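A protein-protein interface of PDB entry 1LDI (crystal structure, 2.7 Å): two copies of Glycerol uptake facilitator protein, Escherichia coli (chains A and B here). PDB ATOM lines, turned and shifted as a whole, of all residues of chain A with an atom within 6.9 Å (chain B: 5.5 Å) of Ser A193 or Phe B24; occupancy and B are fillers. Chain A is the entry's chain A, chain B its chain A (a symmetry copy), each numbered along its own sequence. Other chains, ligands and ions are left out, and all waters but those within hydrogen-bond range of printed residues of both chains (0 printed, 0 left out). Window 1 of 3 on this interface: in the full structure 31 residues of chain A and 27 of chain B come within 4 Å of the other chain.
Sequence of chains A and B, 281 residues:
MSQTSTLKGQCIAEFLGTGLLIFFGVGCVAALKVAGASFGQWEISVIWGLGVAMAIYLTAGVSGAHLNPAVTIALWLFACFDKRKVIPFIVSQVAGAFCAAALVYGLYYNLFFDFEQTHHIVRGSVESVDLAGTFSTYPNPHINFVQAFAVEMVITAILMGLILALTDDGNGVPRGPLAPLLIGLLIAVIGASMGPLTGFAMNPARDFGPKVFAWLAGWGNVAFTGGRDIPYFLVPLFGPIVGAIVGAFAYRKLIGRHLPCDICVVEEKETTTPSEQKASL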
ATOM      1  N   GLN A  41     -20.179   2.978   3.807  1.00  0.00           N
ATOM      2  CA  GLN A  41     -18.799   2.583   4.081  1.00  0.00           C
ATOM      3  C   GLN A  41     -18.128   3.507   5.112  1.00  0.00           C
ATOM      4  O   GLN A  41     -17.385   3.045   5.981  1.00  0.00           O
ATOM      5  CB  GLN A  41     -17.977   2.575   2.794  1.00  0.00           C
ATOM      6  CG  GLN A  41     -16.544   2.092   2.990  1.00  0.00           C
ATOM      7  CD  GLN A  41     -16.485   0.785   3.754  1.00  0.00           C
ATOM      8  OE1 GLN A  41     -17.220  -0.156   3.442  1.00  0.00           O
ATOM      9  NE2 GLN A  41     -15.611   0.713   4.760  1.00  0.00           N
ATOM     10  N   SER A  45     -16.910   2.882   9.116  1.00  0.00           N
ATOM     11  CA  SER A  45     -15.526   3.211   9.378  1.00  0.00           C
ATOM     12  C   SER A  45     -15.371   4.188  10.533  1.00  0.00           C
ATOM     13  O   SER A  45     -14.496   4.023  11.368  1.00  0.00           O
ATOM     14  CB  SER A  45     -14.890   3.799   8.125  1.00  0.00           C
ATOM     15  OG  SER A  45     -14.884   2.842   7.092  1.00  0.00           O
ATOM     16  N   ILE A 155      -1.764  -0.756   4.649  1.00  0.00           N
ATOM     17  CA  ILE A 155      -2.582   0.024   5.569  1.00  0.00           C
ATOM     18  C   ILE A 155      -2.125   0.000   7.023  1.00  0.00           C
ATOM     19  O   ILE A 155      -2.178   1.029   7.694  1.00  0.00           O
ATOM     20  CB  ILE A 155      -4.064  -0.396   5.514  1.00  0.00           C
ATOM     21  CG1 ILE A 155      -4.228  -1.826   6.008  1.00  0.00           C
ATOM     22  CG2 ILE A 155      -4.581  -0.267   4.100  1.00  0.00           C
ATOM     23  CD1 ILE A 155      -5.676  -2.200   6.271  1.00  0.00           C
ATOM     24  N   ILE A 158       0.728   2.283   7.469  1.00  0.00           N
ATOM     25  CA  ILE A 158       0.248   3.650   7.565  1.00  0.00           C
ATOM     26  C   ILE A 158      -0.328   3.892   8.966  1.00  0.00           C
ATOM     27  O   ILE A 158      -0.117   4.945   9.561  1.00  0.00           O
ATOM     28  CB  ILE A 158      -0.833   3.916   6.488  1.00  0.00           C
ATOM     29  CG1 ILE A 158      -0.194   3.851   5.097  1.00  0.00           C
ATOM     30  CG2 ILE A 158      -1.498   5.268   6.722  1.00  0.00           C
ATOM     31  CD1 ILE A 158      -1.145   4.162   3.960  1.00  0.00           C
ATOM     32  N   LEU A 162       1.416   6.697  11.310  1.00  0.00           N
ATOM     33  CA  LEU A 162       0.679   7.873  11.756  1.00  0.00           C
ATOM     34  C   LEU A 162       0.411   7.835  13.248  1.00  0.00           C
ATOM     35  O   LEU A 162       0.278   8.888  13.880  1.00  0.00           O
ATOM     36  CB  LEU A 162      -0.633   8.015  10.983  1.00  0.00           C
ATOM     37  CG  LEU A 162      -0.594   8.889   9.719  1.00  0.00           C
ATOM     38  CD1 LEU A 162      -0.293  10.326  10.099  1.00  0.00           C
ATOM     39  CD2 LEU A 162       0.449   8.378   8.749  1.00  0.00           C
ATOM     40  N   LEU A 185     -10.042   8.923  13.892  1.00  0.00           N
ATOM     41  CA  LEU A 185     -10.397   9.413  12.563  1.00  0.00           C
ATOM     42  C   LEU A 185      -9.456   8.810  11.525  1.00  0.00           C
ATOM     43  O   LEU A 185      -9.868   8.518  10.395  1.00  0.00           O
ATOM     44  CB  LEU A 185     -10.320  10.942  12.515  1.00  0.00           C
ATOM     45  CG  LEU A 185     -11.196  11.709  13.506  1.00  0.00           C
ATOM     46  CD1 LEU A 185     -10.981  13.209  13.337  1.00  0.00           C
ATOM     47  CD2 LEU A 185     -12.652  11.351  13.276  1.00  0.00           C
ATOM     48  N   LEU A 186      -8.189   8.638  11.903  1.00  0.00           N
ATOM     49  CA  LEU A 186      -7.209   8.042  10.998  1.00  0.00           C
ATOM     50  C   LEU A 186      -7.735   6.655  10.642  1.00  0.00           C
ATOM     51  O   LEU A 186      -7.828   6.288   9.466  1.00  0.00           O
ATOM     52  CB  LEU A 186      -5.854   7.913  11.691  1.00  0.00           C
ATOM     53  CG  LEU A 186      -4.830   6.938  11.099  1.00  0.00           C
ATOM     54  CD1 LEU A 186      -4.374   7.417   9.733  1.00  0.00           C
ATOM     55  CD2 LEU A 186      -3.646   6.816  12.057  1.00  0.00           C
ATOM     56  N   ILE A 187      -8.082   5.889  11.672  1.00  0.00           N
ATOM     57  CA  ILE A 187      -8.621   4.559  11.455  1.00  0.00           C
ATOM     58  C   ILE A 187      -9.872   4.681  10.591  1.00  0.00           C
ATOM     59  O   ILE A 187     -10.131   3.842   9.742  1.00  0.00           O
ATOM     60  CB  ILE A 187      -8.975   3.874  12.794  1.00  0.00           C
ATOM     61  CG1 ILE A 187      -7.687   3.417  13.489  1.00  0.00           C
ATOM     62  CG2 ILE A 187      -9.938   2.705  12.551  1.00  0.00           C
ATOM     63  CD1 ILE A 187      -7.900   2.871  14.884  1.00  0.00           C
ATOM     64  N   ALA A 188     -10.636   5.745  10.799  1.00  0.00           N
ATOM     65  CA  ALA A 188     -11.852   5.957  10.037  1.00  0.00           C
ATOM     66  C   ALA A 188     -11.562   6.065   8.547  1.00  0.00           C
ATOM     67  O   ALA A 188     -12.157   5.342   7.744  1.00  0.00           O
ATOM     68  CB  ALA A 188     -12.548   7.207  10.517  1.00  0.00           C
ATOM     69  N   VAL A 189     -10.640   6.954   8.178  1.00  0.00           N
ATOM     70  CA  VAL A 189     -10.316   7.159   6.768  1.00  0.00           C
ATOM     71  C   VAL A 189      -9.647   5.972   6.093  1.00  0.00           C
ATOM     72  O   VAL A 189      -9.799   5.798   4.877  1.00  0.00           O
ATOM     73  CB  VAL A 189      -9.446   8.430   6.549  1.00  0.00           C
ATOM     74  CG1 VAL A 189     -10.171   9.636   7.096  1.00  0.00           C
ATOM     75  CG2 VAL A 189      -8.089   8.280   7.201  1.00  0.00           C
ATOM     76  N   ILE A 190      -8.907   5.166   6.861  1.00  0.00           N
ATOM     77  CA  ILE A 190      -8.262   3.974   6.300  1.00  0.00           C
ATOM     78  C   ILE A 190      -9.393   2.973   6.003  1.00  0.00           C
ATOM     79  O   ILE A 190      -9.388   2.271   4.990  1.00  0.00           O
ATOM     80  CB  ILE A 190      -7.286   3.295   7.309  1.00  0.00           C
ATOM     81  CG1 ILE A 190      -6.090   4.203   7.610  1.00  0.00           C
ATOM     82  CG2 ILE A 190      -6.794   1.977   6.747  1.00  0.00           C
ATOM     83  CD1 ILE A 190      -5.185   3.670   8.719  1.00  0.00           C
ATOM     84  N   GLY A 191     -10.369   2.930   6.901  1.00  0.00           N
ATOM     85  CA  GLY A 191     -11.470   2.015   6.731  1.00  0.00           C
ATOM     86  C   GLY A 191     -12.381   2.405   5.592  1.00  0.00           C
ATOM     87  O   GLY A 191     -13.021   1.544   4.985  1.00  0.00           O
ATOM     88  N   ALA A 192     -12.444   3.695   5.295  1.00  0.00           N
ATOM     89  CA  ALA A 192     -13.308   4.178   4.228  1.00  0.00           C
ATOM     90  C   ALA A 192     -12.636   4.168   2.857  1.00  0.00           C
ATOM     91  O   ALA A 192     -13.304   4.024   1.838  1.00  0.00           O
ATOM     92  CB  ALA A 192     -13.799   5.578   4.564  1.00  0.00           C
ATOM     93  N   SER A 193     -11.314   4.316   2.838  1.00  0.00           N
ATOM     94  CA  SER A 193     -10.551   4.322   1.593  1.00  0.00           C
ATOM     95  C   SER A 193     -10.082   2.931   1.153  1.00  0.00           C
ATOM     96  O   SER A 193      -9.992   2.649  -0.043  1.00  0.00           O
ATOM     97  CB  SER A 193      -9.325   5.237   1.729  1.00  0.00           C
ATOM     98  OG  SER A 193      -8.387   4.726   2.671  1.00  0.00           O
ATOM     99  N   MET A 194      -9.781   2.068   2.121  1.00  0.00           N
ATOM    100  CA  MET A 194      -9.287   0.723   1.832  1.00  0.00           C
ATOM    101  C   MET A 194     -10.162  -0.407   2.364  1.00  0.00           C
ATOM    102  O   MET A 194      -9.930  -1.577   2.057  1.00  0.00           O
ATOM    103  CB  MET A 194      -7.874   0.560   2.400  1.00  0.00           C
ATOM    104  CG  MET A 194      -6.801   1.346   1.662  1.00  0.00           C
ATOM    105  SD  MET A 194      -6.675   0.865  -0.076  1.00  0.00           S
ATOM    106  CE  MET A 194      -6.804   2.440  -0.901  1.00  0.00           C
ATOM    107  N   GLY A 195     -11.163  -0.059   3.161  1.00  0.00           N
ATOM    108  CA  GLY A 195     -12.037  -1.059   3.741  1.00  0.00           C
ATOM    109  C   GLY A 195     -12.656  -2.117   2.838  1.00  0.00           C
ATOM    110  O   GLY A 195     -12.556  -3.303   3.139  1.00  0.00           O
ATOM    111  N   PRO A 196     -13.308  -1.731   1.733  1.00  0.00           N
ATOM    112  CA  PRO A 196     -13.939  -2.687   0.817  1.00  0.00           C
ATOM    113  C   PRO A 196     -13.044  -3.802   0.290  1.00  0.00           C
ATOM    114  O   PRO A 196     -13.537  -4.767  -0.295  1.00  0.00           O
ATOM    115  CB  PRO A 196     -14.455  -1.792  -0.308  1.00  0.00           C
ATOM    116  CG  PRO A 196     -14.760  -0.505   0.408  1.00  0.00           C
ATOM    117  CD  PRO A 196     -13.534  -0.349   1.276  1.00  0.00           C
ATOM    118  N   LEU A 197     -11.731  -3.678   0.482  1.00  0.00           N
ATOM    119  CA  LEU A 197     -10.820  -4.705  -0.009  1.00  0.00           C
ATOM    120  C   LEU A 197     -10.655  -5.888   0.948  1.00  0.00           C
ATOM    121  O   LEU A 197     -10.814  -7.046   0.537  1.00  0.00           O
ATOM    122  CB  LEU A 197      -9.457  -4.094  -0.321  1.00  0.00           C
ATOM    123  CG  LEU A 197      -9.379  -3.203  -1.563  1.00  0.00           C
ATOM    124  CD1 LEU A 197      -7.964  -2.641  -1.668  1.00  0.00           C
ATOM    125  CD2 LEU A 197      -9.744  -3.987  -2.824  1.00  0.00           C
ATOM    126  N   GLY B  19       0.921  12.433  -0.704  1.00  0.00           N
ATOM    127  CA  GLY B  19       0.553  11.073  -1.030  1.00  0.00           C
ATOM    128  C   GLY B  19      -0.474  10.527  -0.053  1.00  0.00           C
ATOM    129  O   GLY B  19      -1.409   9.828  -0.455  1.00  0.00           O
ATOM    130  N   LEU B  20      -0.304  10.836   1.231  1.00  0.00           N
ATOM    131  CA  LEU B  20      -1.224  10.373   2.279  1.00  0.00           C
ATOM    132  C   LEU B  20      -2.608  10.927   1.937  1.00  0.00           C
ATOM    133  O   LEU B  20      -3.608  10.210   1.908  1.00  0.00           O
ATOM    134  CB  LEU B  20      -0.742  10.894   3.643  1.00  0.00           C
ATOM    135  CG  LEU B  20      -1.234  10.382   5.005  1.00  0.00           C
ATOM    136  CD1 LEU B  20      -2.383  11.223   5.484  1.00  0.00           C
ATOM    137  CD2 LEU B  20      -1.620   8.921   4.929  1.00  0.00           C
ATOM    138  N   LEU B  21      -2.622  12.221   1.659  1.00  0.00           N
ATOM    139  CA  LEU B  21      -3.802  12.978   1.285  1.00  0.00           C
ATOM    140  C   LEU B  21      -4.529  12.319   0.097  1.00  0.00           C
ATOM    141  O   LEU B  21      -5.737  12.084   0.151  1.00  0.00           O
ATOM    142  CB  LEU B  21      -3.325  14.390   0.953  1.00  0.00           C
ATOM    143  CG  LEU B  21      -4.099  15.551   0.353  1.00  0.00           C
ATOM    144  CD1 LEU B  21      -3.171  16.773   0.372  1.00  0.00           C
ATOM    145  CD2 LEU B  21      -4.543  15.246  -1.071  1.00  0.00           C
ATOM    146  N   ILE B  22      -3.797  12.014  -0.974  1.00  0.00           N
ATOM    147  CA  ILE B  22      -4.404  11.374  -2.143  1.00  0.00           C
ATOM    148  C   ILE B  22      -4.776   9.911  -1.876  1.00  0.00           C
ATOM    149  O   ILE B  22      -5.694   9.372  -2.502  1.00  0.00           O
ATOM    150  CB  ILE B  22      -3.471  11.431  -3.385  1.00  0.00           C
ATOM    151  CG1 ILE B  22      -3.697  12.730  -4.159  1.00  0.00           C
ATOM    152  CG2 ILE B  22      -3.729  10.249  -4.295  1.00  0.00           C
ATOM    153  CD1 ILE B  22      -2.899  13.900  -3.623  1.00  0.00           C
ATOM    154  N   PHE B  23      -4.064   9.265  -0.956  1.00  0.00           N
ATOM    155  CA  PHE B  23      -4.372   7.878  -0.648  1.00  0.00           C
ATOM    156  C   PHE B  23      -5.826   7.783  -0.165  1.00  0.00           C
ATOM    157  O   PHE B  23      -6.627   7.029  -0.718  1.00  0.00           O
ATOM    158  CB  PHE B  23      -3.419   7.340   0.427  1.00  0.00           C
ATOM    159  CG  PHE B  23      -3.623   5.877   0.738  1.00  0.00           C
ATOM    160  CD1 PHE B  23      -3.171   4.893  -0.141  1.00  0.00           C
ATOM    161  CD2 PHE B  23      -4.304   5.483   1.891  1.00  0.00           C
ATOM    162  CE1 PHE B  23      -3.394   3.535   0.124  1.00  0.00           C
ATOM    163  CE2 PHE B  23      -4.532   4.133   2.164  1.00  0.00           C
ATOM    164  CZ  PHE B  23      -4.076   3.157   1.277  1.00  0.00           C
ATOM    165  N   PHE B  24      -6.154   8.568   0.856  1.00  0.00           N
ATOM    166  CA  PHE B  24      -7.494   8.599   1.434  1.00  0.00           C
ATOM    167  C   PHE B  24      -8.538   9.143   0.457  1.00  0.00           C
ATOM    168  O   PHE B  24      -9.632   8.582   0.327  1.00  0.00           O
ATOM    169  CB  PHE B  24      -7.491   9.469   2.694  1.00  0.00           C
ATOM    170  CG  PHE B  24      -6.651   8.921   3.807  1.00  0.00           C
ATOM    171  CD1 PHE B  24      -5.922   9.778   4.631  1.00  0.00           C
ATOM    172  CD2 PHE B  24      -6.612   7.551   4.067  1.00  0.00           C
ATOM    173  CE1 PHE B  24      -5.173   9.279   5.699  1.00  0.00           C
ATOM    174  CE2 PHE B  24      -5.869   7.049   5.131  1.00  0.00           C
ATOM    175  CZ  PHE B  24      -5.150   7.915   5.948  1.00  0.00           C
ATOM    176  N   GLY B  25      -8.201  10.238  -0.221  1.00  0.00           N
ATOM    177  CA  GLY B  25      -9.135  10.836  -1.158  1.00  0.00           C
ATOM    178  C   GLY B  25      -9.505   9.973  -2.351  1.00  0.00           C
ATOM    179  O   GLY B  25     -10.674   9.645  -2.556  1.00  0.00           O
ATOM    180  N   VAL B  26      -8.510   9.619  -3.154  1.00  0.00           N
ATOM    181  CA  VAL B  26      -8.746   8.785  -4.322  1.00  0.00           C
ATOM    182  C   VAL B  26      -9.296   7.439  -3.862  1.00  0.00           C
ATOM    183  O   VAL B  26     -10.115   6.823  -4.545  1.00  0.00           O
ATOM    184  CB  VAL B  26      -7.438   8.563  -5.120  1.00  0.00           C
ATOM    185  CG1 VAL B  26      -7.681   7.584  -6.270  1.00  0.00           C
ATOM    186  CG2 VAL B  26      -6.918   9.903  -5.651  1.00  0.00           C
ATOM    187  N   GLY B  27      -8.850   6.998  -2.691  1.00  0.00           N
ATOM    188  CA  GLY B  27      -9.307   5.732  -2.156  1.00  0.00           C
ATOM    189  C   GLY B  27     -10.807   5.671  -1.907  1.00  0.00           C
ATOM    190  O   GLY B  27     -11.476   4.743  -2.370  1.00  0.00           O
ATOM    191  N   CYS B  28     -11.353   6.641  -1.175  1.00  0.00           N
ATOM    192  CA  CYS B  28     -12.782   6.615  -0.912  1.00  0.00           C
ATOM    193  C   CYS B  28     -13.560   6.767  -2.219  1.00  0.00           C
ATOM    194  O   CYS B  28     -14.667   6.244  -2.348  1.00  0.00           O
ATOM    195  CB  CYS B  28     -13.188   7.704   0.093  1.00  0.00           C
ATOM    196  SG  CYS B  28     -13.085   9.416  -0.489  1.00  0.00           S
ATOM    197  N   VAL B  29     -12.982   7.453  -3.202  1.00  0.00           N
ATOM    198  CA  VAL B  29     -13.677   7.619  -4.470  1.00  0.00           C
ATOM    199  C   VAL B  29     -13.609   6.352  -5.332  1.00  0.00           C
ATOM    200  O   VAL B  29     -14.439   6.151  -6.212  1.00  0.00           O
ATOM    201  CB  VAL B  29     -13.126   8.815  -5.265  1.00  0.00           C
ATOM    202  CG1 VAL B  29     -13.984   9.039  -6.524  1.00  0.00           C
ATOM    203  CG2 VAL B  29     -13.134  10.067  -4.392  1.00  0.00           C
ATOM    204  N   ALA B  31     -13.723   3.368  -3.928  1.00  0.00           N
ATOM    205  CA  ALA B  31     -14.681   2.524  -3.224  1.00  0.00           C
ATOM    206  C   ALA B  31     -16.093   2.848  -3.696  1.00  0.00           C
ATOM    207  O   ALA B  31     -16.937   1.962  -3.812  1.00  0.00           O
ATOM    208  CB  ALA B  31     -14.576   2.763  -1.738  1.00  0.00           C
ATOM    209  N   ILE B  47     -14.236  12.947   4.100  1.00  0.00           N
ATOM    210  CA  ILE B  47     -13.121  12.020   4.045  1.00  0.00           C
ATOM    211  C   ILE B  47     -11.907  12.742   3.452  1.00  0.00           C
ATOM    212  O   ILE B  47     -10.806  12.655   3.996  1.00  0.00           O
ATOM    213  CB  ILE B  47     -13.493  10.763   3.220  1.00  0.00           C
ATOM    214  CG1 ILE B  47     -14.644  10.023   3.923  1.00  0.00           C
ATOM    215  CG2 ILE B  47     -12.268   9.864   3.051  1.00  0.00           C
ATOM    216  CD1 ILE B  47     -15.336   8.926   3.091  1.00  0.00           C
ATOM    217  N   LEU B  50     -10.709  15.346   6.139  1.00  0.00           N
ATOM    218  CA  LEU B  50      -9.965  14.723   7.226  1.00  0.00           C
ATOM    219  C   LEU B  50      -8.685  14.032   6.763  1.00  0.00           C
ATOM    220  O   LEU B  50      -7.734  13.876   7.535  1.00  0.00           O
ATOM    221  CB  LEU B  50     -10.853  13.724   7.974  1.00  0.00           C
ATOM    222  CG  LEU B  50     -12.071  14.341   8.680  1.00  0.00           C
ATOM    223  CD1 LEU B  50     -12.836  13.252   9.445  1.00  0.00           C
ATOM    224  CD2 LEU B  50     -11.617  15.461   9.628  1.00  0.00           C
ATOM    225  N   GLY B  51      -8.655  13.617   5.505  1.00  0.00           N
ATOM    226  CA  GLY B  51      -7.466  12.963   4.997  1.00  0.00           C
ATOM    227  C   GLY B  51      -6.362  13.992   4.945  1.00  0.00           C
ATOM    228  O   GLY B  51      -5.209  13.716   5.300  1.00  0.00           O
ATOM    229  N   VAL B  52      -6.732  15.188   4.497  1.00  0.00           N
ATOM    230  CA  VAL B  52      -5.796  16.299   4.390  1.00  0.00           C
ATOM    231  C   VAL B  52      -5.346  16.753   5.781  1.00  0.00           C
ATOM    232  O   VAL B  52      -4.231  17.250   5.950  1.00  0.00           O
ATOM    233  CB  VAL B  52      -6.438  17.508   3.654  1.00  0.00           C
ATOM    234  CG1 VAL B  52      -5.552  18.742   3.816  1.00  0.00           C
ATOM    235  CG2 VAL B  52      -6.629  17.183   2.173  1.00  0.00           C
ATOM    236  N   MET B  54      -4.920  14.780   8.407  1.00  0.00           N
ATOM    237  CA  MET B  54      -3.923  13.818   8.868  1.00  0.00           C
ATOM    238  C   MET B  54      -2.608  14.110   8.169  1.00  0.00           C
ATOM    239  O   MET B  54      -1.541  14.066   8.784  1.00  0.00           O
ATOM    240  CB  MET B  54      -4.360  12.390   8.536  1.00  0.00           C
ATOM    241  CG  MET B  54      -5.607  11.942   9.253  1.00  0.00           C
ATOM    242  SD  MET B  54      -5.375  12.021  11.037  1.00  0.00           S
ATOM    243  CE  MET B  54      -7.062  12.516  11.586  1.00  0.00           C
ATOM    244  N   TYR B 108      -6.784  -1.475  -5.697  1.00  0.00           N
ATOM    245  CA  TYR B 108      -8.130  -1.623  -6.256  1.00  0.00           C
ATOM    246  C   TYR B 108      -8.120  -2.193  -7.679  1.00  0.00           C
ATOM    247  O   TYR B 108      -9.179  -2.329  -8.296  1.00  0.00           O
ATOM    248  CB  TYR B 108      -8.845  -0.262  -6.297  1.00  0.00           C
ATOM    249  CG  TYR B 108      -9.544   0.160  -5.017  1.00  0.00           C
ATOM    250  CD1 TYR B 108      -8.849   0.788  -3.978  1.00  0.00           C
ATOM    251  CD2 TYR B 108     -10.913  -0.055  -4.850  1.00  0.00           C
ATOM    252  CE1 TYR B 108      -9.509   1.194  -2.813  1.00  0.00           C
ATOM    253  CE2 TYR B 108     -11.574   0.346  -3.692  1.00  0.00           C
ATOM    254  CZ  TYR B 108     -10.874   0.969  -2.678  1.00  0.00           C
ATOM    255  OH  TYR B 108     -11.544   1.372  -1.541  1.00  0.00           O
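The backbone carbonyl oxygen (O) of Ser A193 is in hydrogen-bond range of the side-chain hydroxyl (OH) of Tyr B108, at 2.5 Å.
O of Gly B27 lies close to O of Ser A193 (3.5 Å).
The side-chain hydroxyl (OG) of Ser A45 is in hydrogen-bond range of the backbone NH (N) of Ala A192, at 3.1 Å.
The side-chain hydroxyl of Ser A193 sits at hydrogen-bond distance from the backbone carbonyl oxygen of Val A189.
O of Ile A190 sits at hydrogen-bond distance from N of Gly A195 (3.5 Å).
The backbone carbonyl oxygen (O) of Phe B24 sits at hydrogen-bond distance from the side-chain sulfur (SG) of Cys B28, at 3.6 Å.
The side-chain sulfur of Cys B28 lies within hydrogen-bond range of the backbone carbonyl oxygen of Gly B25, at 3.2 Å.
O of Gly B27 sits at hydrogen-bond distance from OH of Tyr B108.
Met B54 touches Leu A185.
Leu A186 touches Phe B24.
Val A189 touches Phe B24 (CG2 to CZ, 3.2 Å).
O of Ala A192 touches CA of Cys B28, 3.8 Å away.
O of Ala A192 touches CB of Ala B31 (3.999 Å).
Ser A193 touches Phe B23.
Cys B28 touches Ser A193.
Phe B23 touches Met A194.
Tyr B108 touches Met A194.
Pro A196 touches Ala B31.
Of chain A, only Leu A186 (3.9 Å), Val A189 (3.2 Å), Ile A190 (3.8 Å) and Ser A193 (3.6 Å) come within 4 Å of Phe B24.
Of the printed residues of chain A, Ile B47 touches Ala A192.
Of the printed residues of chain B, Leu A185 touches Met B54.
Of the printed residues of chain B, Ile A158 touches Phe B23 (3.8 Å).
Of the printed residues of chain A, Ala B31 touches Ala A192 (3.999 Å) and Pro A196 (3.9 Å).
Of the 18 printed residues of chain B, 8 touch a printed residue of chain A.
Printed residues of chain B that touch a printed residue of chain A: Phe B23, Phe B24, Gly B27, Cys B28, Ala B31, Ile B47, Met B54 and Tyr B108.
Hydrophobic or aromatic side chains of chain B that line the printed part of chain A: Phe B23, Phe B24, Ala B31, Ile B47, Met B54 and Tyr B108.
Among the printed residues, no Asp or Glu carboxylate lies within 4 Å of a Lys or Arg side-chain nitrogen of the other chain.
No position is printed for both chains.
Of the 17 pairs that touch across the chains among the printed residues, none has its exchanged pair printed and touching as well.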
